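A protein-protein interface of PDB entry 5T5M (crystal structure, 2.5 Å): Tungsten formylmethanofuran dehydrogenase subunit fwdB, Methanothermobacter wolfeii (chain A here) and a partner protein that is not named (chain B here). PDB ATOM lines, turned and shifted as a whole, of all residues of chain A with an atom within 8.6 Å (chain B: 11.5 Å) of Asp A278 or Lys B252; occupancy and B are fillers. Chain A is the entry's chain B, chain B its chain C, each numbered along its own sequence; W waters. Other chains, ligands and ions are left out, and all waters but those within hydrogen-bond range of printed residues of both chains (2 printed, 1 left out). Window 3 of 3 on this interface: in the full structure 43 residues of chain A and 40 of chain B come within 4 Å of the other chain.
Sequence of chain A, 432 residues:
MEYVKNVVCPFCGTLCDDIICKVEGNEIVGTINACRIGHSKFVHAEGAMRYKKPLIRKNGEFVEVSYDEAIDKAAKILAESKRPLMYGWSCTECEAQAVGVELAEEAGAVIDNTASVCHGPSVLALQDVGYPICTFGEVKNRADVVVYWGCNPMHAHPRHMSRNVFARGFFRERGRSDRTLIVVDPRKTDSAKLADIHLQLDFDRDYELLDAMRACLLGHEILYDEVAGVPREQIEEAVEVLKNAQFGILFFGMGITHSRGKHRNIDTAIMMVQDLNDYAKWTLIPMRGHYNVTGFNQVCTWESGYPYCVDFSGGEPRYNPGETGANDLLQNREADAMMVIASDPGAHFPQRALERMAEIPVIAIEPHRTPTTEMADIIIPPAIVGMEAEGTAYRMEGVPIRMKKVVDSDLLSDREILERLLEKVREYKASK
OD1 of Asp A275 lies within salt-bridge range of NZ of Lys B252, 3.98 Å away. The side-chain sulfur (SD) of Met A271 sits close to the side-chain carboxylate (OE2) of Glu B203 (3.5 Å). The guanidinium group of Arg A214 lies within salt-bridge range of the side-chain carboxylate of Glu B203 (3.0 Å). The side-chain carboxylate (OD2) of Asp A278 is in salt-bridge range of the side-chain amino group (NZ) of Lys B252 (3.3 Å).
ND1 of His A220 lies within hydrogen-bond range of O of Leu A218, at 3.4 Å. The side-chain carboxylate (OD2) of Asp B248 lies within hydrogen-bond range of the backbone NH (N) of Glu B203, 2.9 Å away. The backbone carbonyl oxygen of Glu B246 sits close to a ring nitrogen (ND1) of His B249 (3.4 Å). The side-chain sulfur (SD) of Met A271 lies close to the guanidinium group (NH2) of Arg A214 (3.3 Å). OD1 of Asp B248 lies within hydrogen-bond range of N of Ala B250, 3.0 Å away. The backbone carbonyl oxygen (O) of Gly B221 sits at hydrogen-bond distance from the backbone NH (N) of His B249 (2.9 Å).
Among the printed residues, merely in contact across the chains: Leu A218 with Ala B250, Leu A218 with His B249, Arg A214 with Ile B251, Arg A214 with Ala B250, His A220 with His B249, Met A271 with Ile B251, Leu A218 with Lys B252 and Leu A218 with Ile B251.
Of the printed residues of chain B, Leu A218 touches His B249 (3.4 Å), Ala B250 (3.2 Å), Ile B251 (3.9 Å) and Lys B252 (3.8 Å). Of the printed residues of chain B, Met A271 touches Glu B203 and Ile B251. Of the printed residues of chain B, Asp A275 touches Lys B252 (3.9 Å). Of chain B, only Lys B252 (3.3 Å) comes within 4 Å of Asp A278. No residue of chain B comes within 4 Å of Tyr A279. No residue of chain B comes within 4 Å of Ala A280. Gly B201 touches none of the printed residues of chain A. Of the printed residues of chain A, Glu B203 touches Arg A214 and Met A271. Printed residues of chain A within 4 Å of His B249: Leu A218 (3.4 Å) and His A220 (3.7 Å). Of the printed residues of chain A, Ala B250 touches Arg A214 (3.5 Å) and Leu A218 (3.2 Å). Printed residues of chain A within 4 Å of Lys B252: Leu A218, Asp A275 and Asp A278. Gly B253 touches none of the printed residues of chain A. The nearest residue of chain A that does not touch Lys B252 is Arg A214 (6.2 Å). The nearest printed residue of chain B that does not touch Arg A214 is His B249 (4.6 Å).
Hydrophobic or aromatic side chains of chain A within 4 Å of the printed part of chain B: Leu A218, His A220 and Met A271. Of the 22 printed residues of chain B, 5 touch a printed residue of chain A. Hydrophobic or aromatic side chains of chain B within 4 Å of the printed part of chain A: His B249, Ala B250 and Ile B251.
Water W2 lies within hydrogen-bond range of O of Asp A275 (2.7 Å), OD2 of Asp A278 (2.7 Å) and NZ of Lys B252 (3.2 Å). Water W1 lies within hydrogen-bond range of OD2 of Asp A275, NE of Arg A214 and O of Ala B250.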
ATOM      1  N   ARG A 214      15.771 -23.735 -33.222  1.00  0.00           N
ATOM      2  CA  ARG A 214      16.029 -24.239 -31.878  1.00  0.00           C
ATOM      3  C   ARG A 214      14.756 -24.248 -31.042  1.00  0.00           C
ATOM      4  O   ARG A 214      14.479 -25.218 -30.329  1.00  0.00           O
ATOM      5  CB  ARG A 214      17.123 -23.400 -31.214  1.00  0.00           C
ATOM      6  CG  ARG A 214      18.490 -23.594 -31.869  1.00  0.00           C
ATOM      7  CD  ARG A 214      19.567 -22.758 -31.231  1.00  0.00           C
ATOM      8  NE  ARG A 214      19.773 -23.090 -29.823  1.00  0.00           N
ATOM      9  CZ  ARG A 214      20.534 -22.375 -28.998  1.00  0.00           C
ATOM     10  NH1 ARG A 214      21.156 -21.291 -29.440  1.00  0.00           N
ATOM     11  NH2 ARG A 214      20.678 -22.735 -27.732  1.00  0.00           N
ATOM     12  N   LEU A 217      12.517 -26.975 -32.140  1.00  0.00           N
ATOM     13  CA  LEU A 217      13.102 -28.231 -31.686  1.00  0.00           C
ATOM     14  C   LEU A 217      12.727 -28.543 -30.239  1.00  0.00           C
ATOM     15  O   LEU A 217      12.384 -29.687 -29.912  1.00  0.00           O
ATOM     16  CB  LEU A 217      14.619 -28.146 -31.841  1.00  0.00           C
ATOM     17  CG  LEU A 217      15.447 -29.286 -31.274  1.00  0.00           C
ATOM     18  CD1 LEU A 217      15.102 -30.551 -32.012  1.00  0.00           C
ATOM     19  CD2 LEU A 217      16.918 -28.927 -31.396  1.00  0.00           C
ATOM     20  N   LEU A 218      12.803 -27.547 -29.351  1.00  0.00           N
ATOM     21  CA  LEU A 218      12.443 -27.745 -27.949  1.00  0.00           C
ATOM     22  C   LEU A 218      10.942 -27.669 -27.710  1.00  0.00           C
ATOM     23  O   LEU A 218      10.530 -27.486 -26.563  1.00  0.00           O
ATOM     24  CB  LEU A 218      13.144 -26.718 -27.054  1.00  0.00           C
ATOM     25  CG  LEU A 218      14.674 -26.583 -27.128  1.00  0.00           C
ATOM     26  CD1 LEU A 218      15.149 -25.702 -25.984  1.00  0.00           C
ATOM     27  CD2 LEU A 218      15.414 -27.930 -27.118  1.00  0.00           C
ATOM     28  N   HIS A 220       8.534 -25.446 -28.898  1.00  0.00           N
ATOM     29  CA  HIS A 220       7.887 -24.148 -28.787  1.00  0.00           C
ATOM     30  C   HIS A 220       7.391 -23.691 -30.150  1.00  0.00           C
ATOM     31  O   HIS A 220       8.029 -23.943 -31.179  1.00  0.00           O
ATOM     32  CB  HIS A 220       8.842 -23.111 -28.188  1.00  0.00           C
ATOM     33  CG  HIS A 220       9.181 -23.380 -26.754  1.00  0.00           C
ATOM     34  ND1 HIS A 220      10.275 -24.130 -26.375  1.00  0.00           N
ATOM     35  CD2 HIS A 220       8.551 -23.028 -25.606  1.00  0.00           C
ATOM     36  CE1 HIS A 220      10.310 -24.220 -25.056  1.00  0.00           C
ATOM     37  NE2 HIS A 220       9.275 -23.560 -24.566  1.00  0.00           N
ATOM     38  N   LYS A 243      15.695 -34.053 -37.091  1.00  0.00           N
ATOM     39  CA  LYS A 243      15.360 -34.938 -35.977  1.00  0.00           C
ATOM     40  C   LYS A 243      15.296 -36.402 -36.392  1.00  0.00           C
ATOM     41  O   LYS A 243      15.457 -37.285 -35.540  1.00  0.00           O
ATOM     42  CB  LYS A 243      14.022 -34.534 -35.363  1.00  0.00           C
ATOM     43  CG  LYS A 243      14.076 -33.233 -34.589  1.00  0.00           C
ATOM     44  CD  LYS A 243      12.690 -32.709 -34.251  1.00  0.00           C
ATOM     45  CE  LYS A 243      11.993 -33.563 -33.209  1.00  0.00           C
ATOM     46  NZ  LYS A 243      10.620 -33.065 -32.924  1.00  0.00           N
ATOM     47  N   MET A 271      24.815 -24.958 -30.657  1.00  0.00           N
ATOM     48  CA  MET A 271      23.915 -25.391 -29.599  1.00  0.00           C
ATOM     49  C   MET A 271      22.743 -26.173 -30.169  1.00  0.00           C
ATOM     50  O   MET A 271      22.251 -27.111 -29.528  1.00  0.00           O
ATOM     51  CB  MET A 271      23.435 -24.190 -28.788  1.00  0.00           C
ATOM     52  CG  MET A 271      24.515 -23.547 -27.939  1.00  0.00           C
ATOM     53  SD  MET A 271      23.844 -22.440 -26.679  1.00  0.00           S
ATOM     54  CE  MET A 271      23.061 -23.637 -25.584  1.00  0.00           C
ATOM     55  N   MET A 272      22.289 -25.822 -31.371  1.00  0.00           N
ATOM     56  CA  MET A 272      21.269 -26.640 -32.016  1.00  0.00           C
ATOM     57  C   MET A 272      21.781 -28.056 -32.279  1.00  0.00           C
ATOM     58  O   MET A 272      21.069 -29.033 -32.032  1.00  0.00           O
ATOM     59  CB  MET A 272      20.813 -25.997 -33.318  1.00  0.00           C
ATOM     60  CG  MET A 272      19.609 -26.698 -33.936  1.00  0.00           C
ATOM     61  SD  MET A 272      19.134 -25.982 -35.521  1.00  0.00           S
ATOM     62  CE  MET A 272      20.546 -26.328 -36.549  1.00  0.00           C
ATOM     63  N   VAL A 273      23.016 -28.181 -32.793  1.00  0.00           N
ATOM     64  CA  VAL A 273      23.588 -29.497 -33.068  1.00  0.00           C
ATOM     65  C   VAL A 273      23.666 -30.311 -31.787  1.00  0.00           C
ATOM     66  O   VAL A 273      23.287 -31.488 -31.757  1.00  0.00           O
ATOM     67  CB  VAL A 273      24.972 -29.367 -33.738  1.00  0.00           C
ATOM     68  CG1 VAL A 273      25.691 -30.710 -33.797  1.00  0.00           C
ATOM     69  CG2 VAL A 273      24.838 -28.816 -35.149  1.00  0.00           C
ATOM     70  N   GLN A 274      24.169 -29.698 -30.712  1.00  0.00           N
ATOM     71  CA  GLN A 274      24.223 -30.384 -29.423  1.00  0.00           C
ATOM     72  C   GLN A 274      22.850 -30.894 -29.015  1.00  0.00           C
ATOM     73  O   GLN A 274      22.693 -32.067 -28.659  1.00  0.00           O
ATOM     74  CB  GLN A 274      24.784 -29.456 -28.341  1.00  0.00           C
ATOM     75  CG  GLN A 274      26.255 -29.108 -28.523  1.00  0.00           C
ATOM     76  CD  GLN A 274      26.726 -28.006 -27.582  1.00  0.00           C
ATOM     77  OE1 GLN A 274      25.953 -27.144 -27.182  1.00  0.00           O
ATOM     78  NE2 GLN A 274      28.007 -28.035 -27.231  1.00  0.00           N
ATOM     79  N   ASP A 275      21.839 -30.019 -29.057  1.00  0.00           N
ATOM     80  CA  ASP A 275      20.515 -30.396 -28.580  1.00  0.00           C
ATOM     81  C   ASP A 275      19.824 -31.371 -29.520  1.00  0.00           C
ATOM     82  O   ASP A 275      18.927 -32.105 -29.086  1.00  0.00           O
ATOM     83  CB  ASP A 275      19.638 -29.154 -28.381  1.00  0.00           C
ATOM     84  CG  ASP A 275      20.119 -28.267 -27.242  1.00  0.00           C
ATOM     85  OD1 ASP A 275      20.948 -28.714 -26.420  1.00  0.00           O
ATOM     86  OD2 ASP A 275      19.654 -27.107 -27.175  1.00  0.00           O
ATOM     87  N   LEU A 276      20.217 -31.395 -30.792  1.00  0.00           N
ATOM     88  CA  LEU A 276      19.680 -32.393 -31.707  1.00  0.00           C
ATOM     89  C   LEU A 276      20.005 -33.811 -31.250  1.00  0.00           C
ATOM     90  O   LEU A 276      19.271 -34.753 -31.585  1.00  0.00           O
ATOM     91  CB  LEU A 276      20.230 -32.155 -33.114  1.00  0.00           C
ATOM     92  CG  LEU A 276      19.455 -31.111 -33.928  1.00  0.00           C
ATOM     93  CD1 LEU A 276      20.198 -30.770 -35.206  1.00  0.00           C
ATOM     94  CD2 LEU A 276      18.056 -31.604 -34.250  1.00  0.00           C
ATOM     95  N   ASN A 277      21.083 -33.983 -30.476  1.00  0.00           N
ATOM     96  CA  ASN A 277      21.519 -35.315 -30.085  1.00  0.00           C
ATOM     97  C   ASN A 277      20.559 -35.996 -29.123  1.00  0.00           C
ATOM     98  O   ASN A 277      20.709 -37.196 -28.889  1.00  0.00           O
ATOM     99  CB  ASN A 277      22.928 -35.264 -29.485  1.00  0.00           C
ATOM    100  CG  ASN A 277      24.003 -35.352 -30.553  1.00  0.00           C
ATOM    101  OD1 ASN A 277      24.406 -36.445 -30.951  1.00  0.00           O
ATOM    102  ND2 ASN A 277      24.454 -34.202 -31.044  1.00  0.00           N
ATOM    103  N   ASP A 278      19.558 -35.291 -28.593  1.00  0.00           N
ATOM    104  CA  ASP A 278      18.485 -35.973 -27.870  1.00  0.00           C
ATOM    105  C   ASP A 278      17.477 -36.636 -28.799  1.00  0.00           C
ATOM    106  O   ASP A 278      16.664 -37.438 -28.334  1.00  0.00           O
ATOM    107  CB  ASP A 278      17.767 -34.994 -26.941  1.00  0.00           C
ATOM    108  CG  ASP A 278      18.556 -34.729 -25.665  1.00  0.00           C
ATOM    109  OD1 ASP A 278      19.115 -35.706 -25.103  1.00  0.00           O
ATOM    110  OD2 ASP A 278      18.645 -33.549 -25.242  1.00  0.00           O
ATOM    111  N   TYR A 279      17.526 -36.338 -30.087  1.00  0.00           N
ATOM    112  CA  TYR A 279      16.644 -36.935 -31.071  1.00  0.00           C
ATOM    113  C   TYR A 279      17.385 -37.727 -32.132  1.00  0.00           C
ATOM    114  O   TYR A 279      16.831 -38.692 -32.660  1.00  0.00           O
ATOM    115  CB  TYR A 279      15.810 -35.839 -31.756  1.00  0.00           C
ATOM    116  CG  TYR A 279      15.082 -34.948 -30.781  1.00  0.00           C
ATOM    117  CD1 TYR A 279      15.714 -33.855 -30.205  1.00  0.00           C
ATOM    118  CD2 TYR A 279      13.759 -35.192 -30.432  1.00  0.00           C
ATOM    119  CE1 TYR A 279      15.053 -33.030 -29.312  1.00  0.00           C
ATOM    120  CE2 TYR A 279      13.087 -34.364 -29.531  1.00  0.00           C
ATOM    121  CZ  TYR A 279      13.742 -33.291 -28.978  1.00  0.00           C
ATOM    122  OH  TYR A 279      13.097 -32.457 -28.079  1.00  0.00           O
ATOM    123  N   ALA A 280      18.624 -37.358 -32.445  1.00  0.00           N
ATOM    124  CA  ALA A 280      19.368 -37.982 -33.528  1.00  0.00           C
ATOM    125  C   ALA A 280      20.838 -37.635 -33.364  1.00  0.00           C
ATOM    126  O   ALA A 280      21.168 -36.532 -32.931  1.00  0.00           O
ATOM    127  CB  ALA A 280      18.861 -37.507 -34.899  1.00  0.00           C
ATOM    128  N   LYS A 281      21.711 -38.578 -33.713  1.00  0.00           N
ATOM    129  CA  LYS A 281      23.143 -38.337 -33.653  1.00  0.00           C
ATOM    130  C   LYS A 281      23.530 -37.210 -34.597  1.00  0.00           C
ATOM    131  O   LYS A 281      23.254 -37.271 -35.801  1.00  0.00           O
ATOM    132  CB  LYS A 281      23.895 -39.617 -34.015  1.00  0.00           C
ATOM    133  CG  LYS A 281      25.392 -39.472 -34.163  1.00  0.00           C
ATOM    134  CD  LYS A 281      26.069 -39.237 -32.843  1.00  0.00           C
ATOM    135  CE  LYS A 281      27.564 -39.207 -33.043  1.00  0.00           C
ATOM    136  NZ  LYS A 281      28.308 -38.918 -31.794  1.00  0.00           N
ATOM    137  N   TRP A 282      24.200 -36.194 -34.054  1.00  0.00           N
ATOM    138  CA  TRP A 282      24.510 -34.988 -34.808  1.00  0.00           C
ATOM    139  C   TRP A 282      25.873 -34.447 -34.418  1.00  0.00           C
ATOM    140  O   TRP A 282      26.249 -34.458 -33.242  1.00  0.00           O
ATOM    141  CB  TRP A 282      23.444 -33.903 -34.596  1.00  0.00           C
ATOM    142  CG  TRP A 282      22.404 -33.958 -35.626  1.00  0.00           C
ATOM    143  CD1 TRP A 282      21.218 -34.604 -35.547  1.00  0.00           C
ATOM    144  CD2 TRP A 282      22.464 -33.372 -36.931  1.00  0.00           C
ATOM    145  NE1 TRP A 282      20.521 -34.454 -36.726  1.00  0.00           N
ATOM    146  CE2 TRP A 282      21.272 -33.702 -37.591  1.00  0.00           C
ATOM    147  CE3 TRP A 282      23.411 -32.603 -37.601  1.00  0.00           C
ATOM    148  CZ2 TRP A 282      20.999 -33.290 -38.893  1.00  0.00           C
ATOM    149  CZ3 TRP A 282      23.138 -32.190 -38.892  1.00  0.00           C
ATOM    150  CH2 TRP A 282      21.941 -32.536 -39.521  1.00  0.00           C
ATOM    151  N   HIS B 184      23.199 -14.390 -23.926  1.00  0.00           N
ATOM    152  CA  HIS B 184      23.493 -15.408 -22.910  1.00  0.00           C
ATOM    153  C   HIS B 184      23.309 -14.897 -21.487  1.00  0.00           C
ATOM    154  O   HIS B 184      23.879 -15.455 -20.544  1.00  0.00           O
ATOM    155  CB  HIS B 184      24.910 -15.965 -23.070  1.00  0.00           C
ATOM    156  CG  HIS B 184      25.066 -16.895 -24.227  1.00  0.00           C
ATOM    157  ND1 HIS B 184      24.528 -18.163 -24.236  1.00  0.00           N
ATOM    158  CD2 HIS B 184      25.713 -16.750 -25.408  1.00  0.00           C
ATOM    159  CE1 HIS B 184      24.830 -18.757 -25.376  1.00  0.00           C
ATOM    160  NE2 HIS B 184      25.550 -17.922 -26.106  1.00  0.00           N
ATOM    161  N   MET B 185      22.521 -13.843 -21.321  1.00  0.00           N
ATOM    162  CA  MET B 185      22.255 -13.277 -20.004  1.00  0.00           C
ATOM    163  C   MET B 185      21.639 -14.311 -19.070  1.00  0.00           C
ATOM    164  O   MET B 185      20.676 -14.992 -19.426  1.00  0.00           O
ATOM    165  CB  MET B 185      21.316 -12.085 -20.160  1.00  0.00           C
ATOM    166  CG  MET B 185      21.010 -11.366 -18.896  1.00  0.00           C
ATOM    167  SD  MET B 185      19.943  -9.965 -19.218  1.00  0.00           S
ATOM    168  CE  MET B 185      20.062  -9.147 -17.646  1.00  0.00           C
ATOM    169  N   ASN B 186      22.193 -14.417 -17.862  1.00  0.00           N
ATOM    170  CA  ASN B 186      21.631 -15.268 -16.819  1.00  0.00           C
ATOM    171  C   ASN B 186      20.887 -14.483 -15.752  1.00  0.00           C
ATOM    172  O   ASN B 186      19.916 -14.991 -15.183  1.00  0.00           O
ATOM    173  CB  ASN B 186      22.732 -16.090 -16.139  1.00  0.00           C
ATOM    174  CG  ASN B 186      23.139 -17.296 -16.957  1.00  0.00           C
ATOM    175  OD1 ASN B 186      22.298 -18.121 -17.320  1.00  0.00           O
ATOM    176  ND2 ASN B 186      24.425 -17.397 -17.266  1.00  0.00           N
ATOM    177  N   GLY B 201      18.361  -9.956 -26.034  1.00  0.00           N
ATOM    178  CA  GLY B 201      18.061 -11.132 -25.246  1.00  0.00           C
ATOM    179  C   GLY B 201      18.459 -12.440 -25.880  1.00  0.00           C
ATOM    180  O   GLY B 201      18.145 -13.496 -25.321  1.00  0.00           O
ATOM    181  N   GLY B 202      19.138 -12.408 -27.024  1.00  0.00           N
ATOM    182  CA  GLY B 202      19.565 -13.621 -27.694  1.00  0.00           C
ATOM    183  C   GLY B 202      20.113 -14.673 -26.754  1.00  0.00           C
ATOM    184  O   GLY B 202      21.070 -14.416 -26.021  1.00  0.00           O
ATOM    185  N   GLU B 203      19.503 -15.861 -26.760  1.00  0.00           N
ATOM    186  CA  GLU B 203      19.939 -16.989 -25.933  1.00  0.00           C
ATOM    187  C   GLU B 203      20.016 -16.627 -24.451  1.00  0.00           C
ATOM    188  O   GLU B 203      20.829 -17.186 -23.711  1.00  0.00           O
ATOM    189  CB  GLU B 203      21.294 -17.532 -26.404  1.00  0.00           C
ATOM    190  CG  GLU B 203      21.279 -18.082 -27.818  1.00  0.00           C
ATOM    191  CD  GLU B 203      22.665 -18.296 -28.363  1.00  0.00           C
ATOM    192  OE1 GLU B 203      23.270 -17.315 -28.839  1.00  0.00           O
ATOM    193  OE2 GLU B 203      23.158 -19.436 -28.300  1.00  0.00           O
ATOM    194  N   MET B 204      19.187 -15.700 -23.982  1.00  0.00           N
ATOM    195  CA  MET B 204      19.177 -15.414 -22.556  1.00  0.00           C
ATOM    196  C   MET B 204      18.452 -16.529 -21.815  1.00  0.00           C
ATOM    197  O   MET B 204      17.484 -17.107 -22.314  1.00  0.00           O
ATOM    198  CB  MET B 204      18.507 -14.065 -22.271  1.00  0.00           C
ATOM    199  CG  MET B 204      16.987 -14.103 -22.353  1.00  0.00           C
ATOM    200  SD  MET B 204      16.253 -12.467 -22.289  1.00  0.00           S
ATOM    201  CE  MET B 204      16.774 -11.899 -20.670  1.00  0.00           C
ATOM    202  N   ALA B 205      18.954 -16.848 -20.625  1.00  0.00           N
ATOM    203  CA  ALA B 205      18.332 -17.825 -19.744  1.00  0.00           C
ATOM    204  C   ALA B 205      17.567 -17.185 -18.597  1.00  0.00           C
ATOM    205  O   ALA B 205      16.665 -17.817 -18.033  1.00  0.00           O
ATOM    206  CB  ALA B 205      19.404 -18.767 -19.181  1.00  0.00           C
ATOM    207  N   GLY B 206      17.906 -15.951 -18.253  1.00  0.00           N
ATOM    208  CA  GLY B 206      17.226 -15.234 -17.194  1.00  0.00           C
ATOM    209  C   GLY B 206      17.648 -13.779 -17.208  1.00  0.00           C
ATOM    210  O   GLY B 206      18.380 -13.329 -18.091  1.00  0.00           O
ATOM    211  N   GLY B 207      17.187 -13.041 -16.206  1.00  0.00           N
ATOM    212  CA  GLY B 207      17.451 -11.616 -16.161  1.00  0.00           C
ATOM    213  C   GLY B 207      16.376 -10.829 -16.882  1.00  0.00           C
ATOM    214  O   GLY B 207      15.396 -11.372 -17.402  1.00  0.00           O
ATOM    215  N   GLY B 221      12.045 -16.849 -30.769  1.00  0.00           N
ATOM    216  CA  GLY B 221      12.065 -17.719 -29.616  1.00  0.00           C
ATOM    217  C   GLY B 221      11.512 -17.121 -28.343  1.00  0.00           C
ATOM    218  O   GLY B 221      11.575 -17.768 -27.295  1.00  0.00           O
ATOM    219  N   GLU B 246       8.954 -13.419 -22.846  1.00  0.00           N
ATOM    220  CA  GLU B 246       9.706 -14.406 -22.084  1.00  0.00           C
ATOM    221  C   GLU B 246      10.495 -15.301 -23.031  1.00  0.00           C
ATOM    222  O   GLU B 246       9.974 -15.742 -24.059  1.00  0.00           O
ATOM    223  CB  GLU B 246       8.775 -15.259 -21.226  1.00  0.00           C
ATOM    224  CG  GLU B 246       9.491 -16.199 -20.296  1.00  0.00           C
ATOM    225  CD  GLU B 246       8.551 -17.210 -19.661  1.00  0.00           C
ATOM    226  OE1 GLU B 246       7.785 -17.863 -20.409  1.00  0.00           O
ATOM    227  OE2 GLU B 246       8.576 -17.346 -18.419  1.00  0.00           O
ATOM    228  N   GLY B 247      11.747 -15.573 -22.678  1.00  0.00           N
ATOM    229  CA  GLY B 247      12.625 -16.369 -23.524  1.00  0.00           C
ATOM    230  C   GLY B 247      14.027 -16.412 -22.947  1.00  0.00           C
ATOM    231  O   GLY B 247      14.189 -16.152 -21.751  1.00  0.00           O
ATOM    232  N   ASP B 248      15.051 -16.746 -23.740  1.00  0.00           N
ATOM    233  CA  ASP B 248      14.950 -17.180 -25.140  1.00  0.00           C
ATOM    234  C   ASP B 248      14.733 -18.690 -25.145  1.00  0.00           C
ATOM    235  O   ASP B 248      15.583 -19.438 -24.678  1.00  0.00           O
ATOM    236  CB  ASP B 248      16.230 -16.796 -25.908  1.00  0.00           C
ATOM    237  CG  ASP B 248      16.219 -17.227 -27.385  1.00  0.00           C
ATOM    238  OD1 ASP B 248      15.321 -17.979 -27.829  1.00  0.00           O
ATOM    239  OD2 ASP B 248      17.146 -16.816 -28.106  1.00  0.00           O
ATOM    240  N   HIS B 249      13.597 -19.144 -25.670  1.00  0.00           N
ATOM    241  CA  HIS B 249      13.225 -20.544 -25.538  1.00  0.00           C
ATOM    242  C   HIS B 249      13.962 -21.462 -26.509  1.00  0.00           C
ATOM    243  O   HIS B 249      13.655 -22.656 -26.548  1.00  0.00           O
ATOM    244  CB  HIS B 249      11.706 -20.697 -25.675  1.00  0.00           C
ATOM    245  CG  HIS B 249      10.971 -20.209 -24.464  1.00  0.00           C
ATOM    246  ND1 HIS B 249      10.108 -19.132 -24.490  1.00  0.00           N
ATOM    247  CD2 HIS B 249      11.027 -20.616 -23.173  1.00  0.00           C
ATOM    248  CE1 HIS B 249       9.646 -18.914 -23.270  1.00  0.00           C
ATOM    249  NE2 HIS B 249      10.188 -19.800 -22.453  1.00  0.00           N
ATOM    250  N   ALA B 250      14.937 -20.946 -27.258  1.00  0.00           N
ATOM    251  CA  ALA B 250      15.990 -21.805 -27.785  1.00  0.00           C
ATOM    252  C   ALA B 250      16.807 -22.430 -26.654  1.00  0.00           C
ATOM    253  O   ALA B 250      17.373 -23.514 -26.829  1.00  0.00           O
ATOM    254  CB  ALA B 250      16.899 -21.004 -28.707  1.00  0.00           C
ATOM    255  N   ILE B 251      16.877 -21.757 -25.494  1.00  0.00           N
ATOM    256  CA  ILE B 251      17.573 -22.252 -24.310  1.00  0.00           C
ATOM    257  C   ILE B 251      16.594 -23.054 -23.468  1.00  0.00           C
ATOM    258  O   ILE B 251      15.418 -22.696 -23.346  1.00  0.00           O
ATOM    259  CB  ILE B 251      18.166 -21.083 -23.500  1.00  0.00           C
ATOM    260  CG1 ILE B 251      19.233 -20.327 -24.310  1.00  0.00           C
ATOM    261  CG2 ILE B 251      18.722 -21.567 -22.169  1.00  0.00           C
ATOM    262  CD1 ILE B 251      20.495 -21.141 -24.664  1.00  0.00           C
ATOM    263  N   LYS B 252      17.083 -24.136 -22.864  1.00  0.00           N
ATOM    264  CA  LYS B 252      16.251 -24.978 -22.015  1.00  0.00           C
ATOM    265  C   LYS B 252      16.022 -24.309 -20.663  1.00  0.00           C
ATOM    266  O   LYS B 252      16.962 -23.801 -20.045  1.00  0.00           O
ATOM    267  CB  LYS B 252      16.901 -26.346 -21.817  1.00  0.00           C
ATOM    268  CG  LYS B 252      17.073 -27.156 -23.096  1.00  0.00           C
ATOM    269  CD  LYS B 252      17.772 -28.468 -22.829  1.00  0.00           C
ATOM    270  CE  LYS B 252      17.862 -29.309 -24.081  1.00  0.00           C
ATOM    271  NZ  LYS B 252      18.580 -30.602 -23.838  1.00  0.00           N
ATOM    272  N   GLY B 253      14.772 -24.327 -20.201  1.00  0.00           N
ATOM    273  CA  GLY B 253      14.420 -23.731 -18.926  1.00  0.00           C
ATOM    274  C   GLY B 253      14.501 -22.221 -18.830  1.00  0.00           C
ATOM    275  O   GLY B 253      14.511 -21.693 -17.718  1.00  0.00           O
ATOM    276  N   ALA B 254      14.529 -21.510 -19.954  1.00  0.00           N
ATOM    277  CA  ALA B 254      14.785 -20.072 -19.939  1.00  0.00           C
ATOM    278  C   ALA B 254      13.660 -19.280 -19.273  1.00  0.00           C
ATOM    279  O   ALA B 254      12.469 -19.520 -19.501  1.00  0.00           O
ATOM    280  CB  ALA B 254      14.987 -19.568 -21.365  1.00  0.00           C
ATOM    281  N   LYS B 255      14.063 -18.298 -18.470  1.00  0.00           N
ATOM    282  CA  LYS B 255      13.150 -17.454 -17.702  1.00  0.00           C
ATOM    283  C   LYS B 255      13.372 -15.971 -17.963  1.00  0.00           C
ATOM    284  O   LYS B 255      12.863 -15.142 -17.207  1.00  0.00           O
ATOM    285  CB  LYS B 255      13.309 -17.719 -16.198  1.00  0.00           C
ATOM    286  CG  LYS B 255      12.973 -19.114 -15.774  1.00  0.00           C
ATOM    287  CD  LYS B 255      11.469 -19.332 -15.891  1.00  0.00           C
ATOM    288  CE  LYS B 255      11.021 -20.656 -15.279  1.00  0.00           C
ATOM    289  NZ  LYS B 255       9.558 -20.869 -15.487  1.00  0.00           N
ATOM    290  N   GLY B 256      14.130 -15.613 -18.992  1.00  0.00           N
ATOM    291  CA  GLY B 256      14.420 -14.218 -19.233  1.00  0.00           C
ATOM    292  C   GLY B 256      13.176 -13.435 -19.604  1.00  0.00           C
ATOM    293  O   GLY B 256      12.209 -13.979 -20.137  1.00  0.00           O
HETATM  294  O   HOH W   1      18.427 -25.416 -28.940  1.00  0.00           O
HETATM  295  O   HOH W   2      17.700 -31.477 -26.764  1.00  0.00           O
